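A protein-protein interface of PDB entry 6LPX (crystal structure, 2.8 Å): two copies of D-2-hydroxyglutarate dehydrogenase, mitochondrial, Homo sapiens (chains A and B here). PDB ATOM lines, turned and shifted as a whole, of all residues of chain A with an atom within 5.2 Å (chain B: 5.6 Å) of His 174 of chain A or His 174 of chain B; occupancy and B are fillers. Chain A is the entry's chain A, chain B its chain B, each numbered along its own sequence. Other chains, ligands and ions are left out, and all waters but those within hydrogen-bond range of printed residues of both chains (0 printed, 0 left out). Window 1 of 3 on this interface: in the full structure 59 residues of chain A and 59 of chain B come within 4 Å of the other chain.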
ATOM      1  N   ASN A 161     -19.281 -21.006 -29.990  1.00  0.00           N
ATOM      2  CA  ASN A 161     -19.863 -22.126 -30.736  1.00  0.00           C
ATOM      3  C   ASN A 161     -19.210 -22.252 -32.124  1.00  0.00           C
ATOM      4  O   ASN A 161     -19.865 -22.216 -33.168  1.00  0.00           O
ATOM      5  CB  ASN A 161     -21.388 -21.997 -30.859  1.00  0.00           C
ATOM      6  CG  ASN A 161     -22.033 -23.211 -31.547  1.00  0.00           C
ATOM      7  OD1 ASN A 161     -21.617 -24.354 -31.360  1.00  0.00           O
ATOM      8  ND2 ASN A 161     -23.033 -22.956 -32.362  1.00  0.00           N
ATOM      9  N   SER A 172     -21.924 -30.067 -34.402  1.00  0.00           N
ATOM     10  CA  SER A 172     -21.844 -28.898 -33.544  1.00  0.00           C
ATOM     11  C   SER A 172     -21.266 -29.230 -32.171  1.00  0.00           C
ATOM     12  O   SER A 172     -21.364 -30.359 -31.692  1.00  0.00           O
ATOM     13  CB  SER A 172     -23.246 -28.297 -33.398  1.00  0.00           C
ATOM     14  OG  SER A 172     -23.259 -27.203 -32.506  1.00  0.00           O
ATOM     15  N   LEU A 173     -20.635 -28.227 -31.549  1.00  0.00           N
ATOM     16  CA  LEU A 173     -20.288 -28.335 -30.132  1.00  0.00           C
ATOM     17  C   LEU A 173     -21.530 -28.524 -29.273  1.00  0.00           C
ATOM     18  O   LEU A 173     -21.444 -29.076 -28.170  1.00  0.00           O
ATOM     19  CB  LEU A 173     -19.516 -27.099 -29.666  1.00  0.00           C
ATOM     20  CG  LEU A 173     -18.108 -26.949 -30.251  1.00  0.00           C
ATOM     21  CD1 LEU A 173     -17.530 -25.558 -29.983  1.00  0.00           C
ATOM     22  CD2 LEU A 173     -17.184 -28.058 -29.768  1.00  0.00           C
ATOM     23  N   HIS A 174     -22.683 -28.033 -29.734  1.00  0.00           N
ATOM     24  CA  HIS A 174     -23.933 -28.344 -29.053  1.00  0.00           C
ATOM     25  C   HIS A 174     -24.161 -29.849 -28.937  1.00  0.00           C
ATOM     26  O   HIS A 174     -24.841 -30.297 -28.010  1.00  0.00           O
ATOM     27  CB  HIS A 174     -25.116 -27.658 -29.755  1.00  0.00           C
ATOM     28  CG  HIS A 174     -25.148 -26.169 -29.577  1.00  0.00           C
ATOM     29  ND1 HIS A 174     -25.467 -25.578 -28.372  1.00  0.00           N
ATOM     30  CD2 HIS A 174     -24.886 -25.155 -30.434  1.00  0.00           C
ATOM     31  CE1 HIS A 174     -25.410 -24.264 -28.499  1.00  0.00           C
ATOM     32  NE2 HIS A 174     -25.061 -23.980 -29.741  1.00  0.00           N
ATOM     33  N   GLY A 175     -23.616 -30.639 -29.853  1.00  0.00           N
ATOM     34  CA  GLY A 175     -23.685 -32.073 -29.704  1.00  0.00           C
ATOM     35  C   GLY A 175     -22.489 -32.735 -29.050  1.00  0.00           C
ATOM     36  O   GLY A 175     -22.652 -33.710 -28.314  1.00  0.00           O
ATOM     37  N   THR A 176     -21.283 -32.226 -29.304  1.00  0.00           N
ATOM     38  CA  THR A 176     -20.070 -32.899 -28.857  1.00  0.00           C
ATOM     39  C   THR A 176     -19.593 -32.467 -27.477  1.00  0.00           C
ATOM     40  O   THR A 176     -18.819 -33.200 -26.853  1.00  0.00           O
ATOM     41  CB  THR A 176     -18.930 -32.693 -29.856  1.00  0.00           C
ATOM     42  OG1 THR A 176     -18.675 -31.291 -30.008  1.00  0.00           O
ATOM     43  CG2 THR A 176     -19.303 -33.277 -31.200  1.00  0.00           C
ATOM     44  N   VAL A 177     -19.997 -31.300 -26.987  1.00  0.00           N
ATOM     45  CA  VAL A 177     -19.624 -30.912 -25.631  1.00  0.00           C
ATOM     46  C   VAL A 177     -20.504 -31.681 -24.657  1.00  0.00           C
ATOM     47  O   VAL A 177     -21.735 -31.605 -24.724  1.00  0.00           O
ATOM     48  CB  VAL A 177     -19.745 -29.396 -25.422  1.00  0.00           C
ATOM     49  CG1 VAL A 177     -19.587 -29.037 -23.944  1.00  0.00           C
ATOM     50  CG2 VAL A 177     -18.684 -28.703 -26.219  1.00  0.00           C
ATOM     51  N   ASP A 204     -30.735 -28.874 -19.934  1.00  0.00           N
ATOM     52  CA  ASP A 204     -29.370 -28.953 -20.433  1.00  0.00           C
ATOM     53  C   ASP A 204     -28.747 -27.558 -20.339  1.00  0.00           C
ATOM     54  O   ASP A 204     -28.496 -26.871 -21.329  1.00  0.00           O
ATOM     55  CB  ASP A 204     -29.357 -29.509 -21.849  1.00  0.00           C
ATOM     56  CG  ASP A 204     -27.987 -30.021 -22.253  1.00  0.00           C
ATOM     57  OD1 ASP A 204     -27.033 -29.844 -21.456  1.00  0.00           O
ATOM     58  OD2 ASP A 204     -27.869 -30.624 -23.349  1.00  0.00           O
ATOM     59  N   GLN A 207     -25.923 -25.797 -22.456  1.00  0.00           N
ATOM     60  CA  GLN A 207     -26.254 -25.280 -23.779  1.00  0.00           C
ATOM     61  C   GLN A 207     -26.370 -23.756 -23.797  1.00  0.00           C
ATOM     62  O   GLN A 207     -26.011 -23.119 -24.794  1.00  0.00           O
ATOM     63  CB  GLN A 207     -27.553 -25.915 -24.265  1.00  0.00           C
ATOM     64  CG  GLN A 207     -27.483 -27.418 -24.488  1.00  0.00           C
ATOM     65  CD  GLN A 207     -26.608 -27.776 -25.666  1.00  0.00           C
ATOM     66  OE1 GLN A 207     -26.139 -26.897 -26.388  1.00  0.00           O
ATOM     67  NE2 GLN A 207     -26.445 -29.065 -25.913  1.00  0.00           N
ATOM     68  N   ILE A 210     -22.899 -22.293 -24.594  1.00  0.00           N
ATOM     69  CA  ILE A 210     -22.244 -22.580 -25.859  1.00  0.00           C
ATOM     70  C   ILE A 210     -22.782 -21.573 -26.862  1.00  0.00           C
ATOM     71  O   ILE A 210     -23.947 -21.647 -27.261  1.00  0.00           O
ATOM     72  CB  ILE A 210     -22.516 -24.020 -26.305  1.00  0.00           C
ATOM     73  CG1 ILE A 210     -22.064 -25.006 -25.222  1.00  0.00           C
ATOM     74  CG2 ILE A 210     -21.830 -24.302 -27.648  1.00  0.00           C
ATOM     75  CD1 ILE A 210     -22.499 -26.404 -25.489  1.00  0.00           C
ATOM     76  N   GLY A 211     -21.918 -20.670 -27.313  1.00  0.00           N
ATOM     77  CA  GLY A 211     -22.346 -19.553 -28.123  1.00  0.00           C
ATOM     78  C   GLY A 211     -22.755 -18.298 -27.364  1.00  0.00           C
ATOM     79  O   GLY A 211     -23.241 -17.356 -27.994  1.00  0.00           O
ATOM     80  N   ASN B 161     -35.976 -34.855 -25.164  1.00  0.00           N
ATOM     81  CA  ASN B 161     -34.641 -35.115 -25.715  1.00  0.00           C
ATOM     82  C   ASN B 161     -34.393 -36.615 -25.904  1.00  0.00           C
ATOM     83  O   ASN B 161     -33.419 -37.177 -25.418  1.00  0.00           O
ATOM     84  CB  ASN B 161     -33.567 -34.460 -24.836  1.00  0.00           C
ATOM     85  CG  ASN B 161     -32.164 -34.637 -25.377  1.00  0.00           C
ATOM     86  OD1 ASN B 161     -31.930 -34.639 -26.591  1.00  0.00           O
ATOM     87  ND2 ASN B 161     -31.211 -34.764 -24.468  1.00  0.00           N
ATOM     88  N   SER B 172     -27.405 -36.488 -30.667  1.00  0.00           N
ATOM     89  CA  SER B 172     -28.463 -35.881 -29.883  1.00  0.00           C
ATOM     90  C   SER B 172     -29.365 -34.989 -30.734  1.00  0.00           C
ATOM     91  O   SER B 172     -28.969 -34.486 -31.789  1.00  0.00           O
ATOM     92  CB  SER B 172     -27.823 -35.059 -28.759  1.00  0.00           C
ATOM     93  OG  SER B 172     -28.754 -34.338 -27.990  1.00  0.00           O
ATOM     94  N   LEU B 173     -30.620 -34.849 -30.283  1.00  0.00           N
ATOM     95  CA  LEU B 173     -31.519 -33.820 -30.802  1.00  0.00           C
ATOM     96  C   LEU B 173     -30.983 -32.420 -30.562  1.00  0.00           C
ATOM     97  O   LEU B 173     -31.339 -31.492 -31.290  1.00  0.00           O
ATOM     98  CB  LEU B 173     -32.914 -33.955 -30.193  1.00  0.00           C
ATOM     99  CG  LEU B 173     -33.716 -35.172 -30.636  1.00  0.00           C
ATOM    100  CD1 LEU B 173     -34.993 -35.310 -29.819  1.00  0.00           C
ATOM    101  CD2 LEU B 173     -34.004 -35.059 -32.118  1.00  0.00           C
ATOM    102  N   HIS B 174     -30.185 -32.237 -29.505  1.00  0.00           N
ATOM    103  CA  HIS B 174     -29.496 -30.968 -29.298  1.00  0.00           C
ATOM    104  C   HIS B 174     -28.632 -30.610 -30.494  1.00  0.00           C
ATOM    105  O   HIS B 174     -28.329 -29.433 -30.703  1.00  0.00           O
ATOM    106  CB  HIS B 174     -28.654 -31.017 -28.018  1.00  0.00           C
ATOM    107  CG  HIS B 174     -29.462 -31.042 -26.750  1.00  0.00           C
ATOM    108  ND1 HIS B 174     -30.100 -29.926 -26.245  1.00  0.00           N
ATOM    109  CD2 HIS B 174     -29.750 -32.054 -25.895  1.00  0.00           C
ATOM    110  CE1 HIS B 174     -30.739 -30.249 -25.134  1.00  0.00           C
ATOM    111  NE2 HIS B 174     -30.545 -31.536 -24.901  1.00  0.00           N
ATOM    112  N   GLY B 175     -28.188 -31.606 -31.261  1.00  0.00           N
ATOM    113  CA  GLY B 175     -27.498 -31.355 -32.514  1.00  0.00           C
ATOM    114  C   GLY B 175     -28.331 -31.347 -33.780  1.00  0.00           C
ATOM    115  O   GLY B 175     -28.066 -30.539 -34.671  1.00  0.00           O
ATOM    116  N   THR B 176     -29.343 -32.209 -33.882  1.00  0.00           N
ATOM    117  CA  THR B 176     -30.059 -32.377 -35.146  1.00  0.00           C
ATOM    118  C   THR B 176     -31.272 -31.469 -35.290  1.00  0.00           C
ATOM    119  O   THR B 176     -31.773 -31.304 -36.407  1.00  0.00           O
ATOM    120  CB  THR B 176     -30.484 -33.842 -35.345  1.00  0.00           C
ATOM    121  OG1 THR B 176     -31.218 -34.309 -34.211  1.00  0.00           O
ATOM    122  CG2 THR B 176     -29.253 -34.725 -35.504  1.00  0.00           C
ATOM    123  N   VAL B 177     -31.811 -30.952 -34.190  1.00  0.00           N
ATOM    124  CA  VAL B 177     -32.878 -29.964 -34.279  1.00  0.00           C
ATOM    125  C   VAL B 177     -32.258 -28.648 -34.721  1.00  0.00           C
ATOM    126  O   VAL B 177     -31.352 -28.119 -34.071  1.00  0.00           O
ATOM    127  CB  VAL B 177     -33.615 -29.820 -32.940  1.00  0.00           C
ATOM    128  CG1 VAL B 177     -34.593 -28.669 -33.003  1.00  0.00           C
ATOM    129  CG2 VAL B 177     -34.351 -31.116 -32.597  1.00  0.00           C
ATOM    130  N   ASP B 204     -28.511 -19.552 -28.231  1.00  0.00           N
ATOM    131  CA  ASP B 204     -29.210 -20.676 -28.842  1.00  0.00           C
ATOM    132  C   ASP B 204     -30.414 -21.046 -27.965  1.00  0.00           C
ATOM    133  O   ASP B 204     -30.428 -22.040 -27.240  1.00  0.00           O
ATOM    134  CB  ASP B 204     -28.240 -21.828 -29.034  1.00  0.00           C
ATOM    135  CG  ASP B 204     -28.706 -22.792 -30.073  1.00  0.00           C
ATOM    136  OD1 ASP B 204     -29.787 -22.532 -30.653  1.00  0.00           O
ATOM    137  OD2 ASP B 204     -27.969 -23.772 -30.341  1.00  0.00           O
ATOM    138  N   LYS B 206     -33.368 -22.214 -28.458  1.00  0.00           N
ATOM    139  CA  LYS B 206     -34.079 -23.475 -28.645  1.00  0.00           C
ATOM    140  C   LYS B 206     -33.518 -24.574 -27.760  1.00  0.00           C
ATOM    141  O   LYS B 206     -34.267 -25.456 -27.320  1.00  0.00           O
ATOM    142  CB  LYS B 206     -34.033 -23.897 -30.110  1.00  0.00           C
ATOM    143  CG  LYS B 206     -32.653 -24.375 -30.561  1.00  0.00           C
ATOM    144  CD  LYS B 206     -32.649 -24.869 -32.001  1.00  0.00           C
ATOM    145  CE  LYS B 206     -31.270 -25.331 -32.408  1.00  0.00           C
ATOM    146  NZ  LYS B 206     -30.470 -24.158 -32.796  1.00  0.00           N
ATOM    147  N   GLN B 207     -32.225 -24.510 -27.445  1.00  0.00           N
ATOM    148  CA  GLN B 207     -31.623 -25.550 -26.627  1.00  0.00           C
ATOM    149  C   GLN B 207     -32.320 -25.666 -25.282  1.00  0.00           C
ATOM    150  O   GLN B 207     -32.417 -26.760 -24.714  1.00  0.00           O
ATOM    151  CB  GLN B 207     -30.143 -25.252 -26.424  1.00  0.00           C
ATOM    152  CG  GLN B 207     -29.318 -25.282 -27.690  1.00  0.00           C
ATOM    153  CD  GLN B 207     -29.342 -26.642 -28.370  1.00  0.00           C
ATOM    154  OE1 GLN B 207     -29.663 -27.670 -27.747  1.00  0.00           O
ATOM    155  NE2 GLN B 207     -29.001 -26.658 -29.658  1.00  0.00           N
ATOM    156  N   ILE B 210     -35.205 -28.220 -25.490  1.00  0.00           N
ATOM    157  CA  ILE B 210     -34.884 -29.616 -25.763  1.00  0.00           C
ATOM    158  C   ILE B 210     -34.568 -30.274 -24.426  1.00  0.00           C
ATOM    159  O   ILE B 210     -33.574 -29.941 -23.777  1.00  0.00           O
ATOM    160  CB  ILE B 210     -33.715 -29.734 -26.738  1.00  0.00           C
ATOM    161  CG1 ILE B 210     -34.072 -28.988 -28.025  1.00  0.00           C
ATOM    162  CG2 ILE B 210     -33.424 -31.194 -27.022  1.00  0.00           C
ATOM    163  CD1 ILE B 210     -32.979 -28.999 -29.030  1.00  0.00           C
ATOM    164  N   GLY B 211     -35.407 -31.221 -24.024  1.00  0.00           N
ATOM    165  CA  GLY B 211     -35.266 -31.870 -22.739  1.00  0.00           C
ATOM    166  C   GLY B 211     -35.950 -31.173 -21.581  1.00  0.00           C
ATOM    167  O   GLY B 211     -35.782 -31.616 -20.437  1.00  0.00           O
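NE2 of His 174 of chain A sits at hydrogen-bond distance from OD2 of Asp 204 of chain B (3.0 Å). The side-chain carboxylate (OD2) of Asp 204 of chain A sits at hydrogen-bond distance from a ring nitrogen (NE2) of His 174 of chain B (3.2 Å).
The side-chain amide nitrogen (ND2) of Asn 161 of chain A lies close to a ring nitrogen (NE2) of His 174 of chain A. The backbone NH (N) of His 174 of chain A is in hydrogen-bond range of the side-chain hydroxyl (OG) of Ser 172 of chain A (3.0 Å). The side-chain amide nitrogen of Asn 161 of chain B lies within hydrogen-bond range of a ring nitrogen (NE2) of His 174 of chain B (3.3 Å). OE1 of Gln 207 of chain B sits at hydrogen-bond distance from ND1 of His 174 of chain B, at 2.7 Å. The side-chain carboxylate of Asp 204 of chain B is in salt-bridge range of the side-chain amino group of Lys 206 of chain B, at 2.8 Å. OD2 of Asp 204 of chain B sits at hydrogen-bond distance from NE2 of Gln 207 of chain B (3.1 Å).
His 174 of chain A touches His 174 of chain B. NE2 of Gln 207 of chain B touches CG of His 174 of chain A, 3.9 Å away. Gln 207 of chain A touches His 174 of chain B. Gln 207 of chain A touches Gln 207 of chain B (CB to CB, 3.4 Å).
His 174 of chain A touches just these residues of chain B: His 174 (3.8 Å), Asp 204 (3.0 Å) and Gln 207 (3.9 Å). His 174 of chain B touches three residues of chain A. Of the printed residues of chain A, Asp 204 of chain B touches His 174. Printed residues of chain B within 4 Å of Asp 204 of chain A: His 174 (3.2 Å). Ile 210 of chain B touches none of the printed residues of chain A. Leu 173 of chain B touches none of the printed residues of chain A. The nearest residue of chain B that does not touch His 174 of chain A is Gly 175 of chain B (4.8 Å). The nearest residue of chain A that does not touch His 174 of chain B is Gly 175 of chain A (4.9 Å). The nearest printed residue of chain B that does not touch Asp 204 of chain A is Ile 210 of chain B (4.7 Å).
Of the 12 printed residues of chain B, 3 touch a printed residue of chain A. Hydrophobic or aromatic side chains of chain B within 4 Å of the printed part of chain A: His 174. Among the printed residues, 6 pairs touch across the chains. Among the printed residues, no Asp or Glu carboxylate lies within 4 Å of a Lys or Arg side-chain nitrogen of the other chain.
His 174 of chain B touches its own counterpart, His 174 of chain A. His 174 of chain A touches Asp 204 of chain B, and with the chains exchanged Asp 204 of chain A touches His 174 of chain B. His 174 of chain A touches Gln 207 of chain B, and with the chains exchanged Gln 207 of chain A touches His 174 of chain B. Gln 207 of chain B touches its own counterpart, Gln 207 of chain A. Of the 6 pairs that touch across the chains among the printed residues, 6 have their exchanged pair printed and touching as well.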
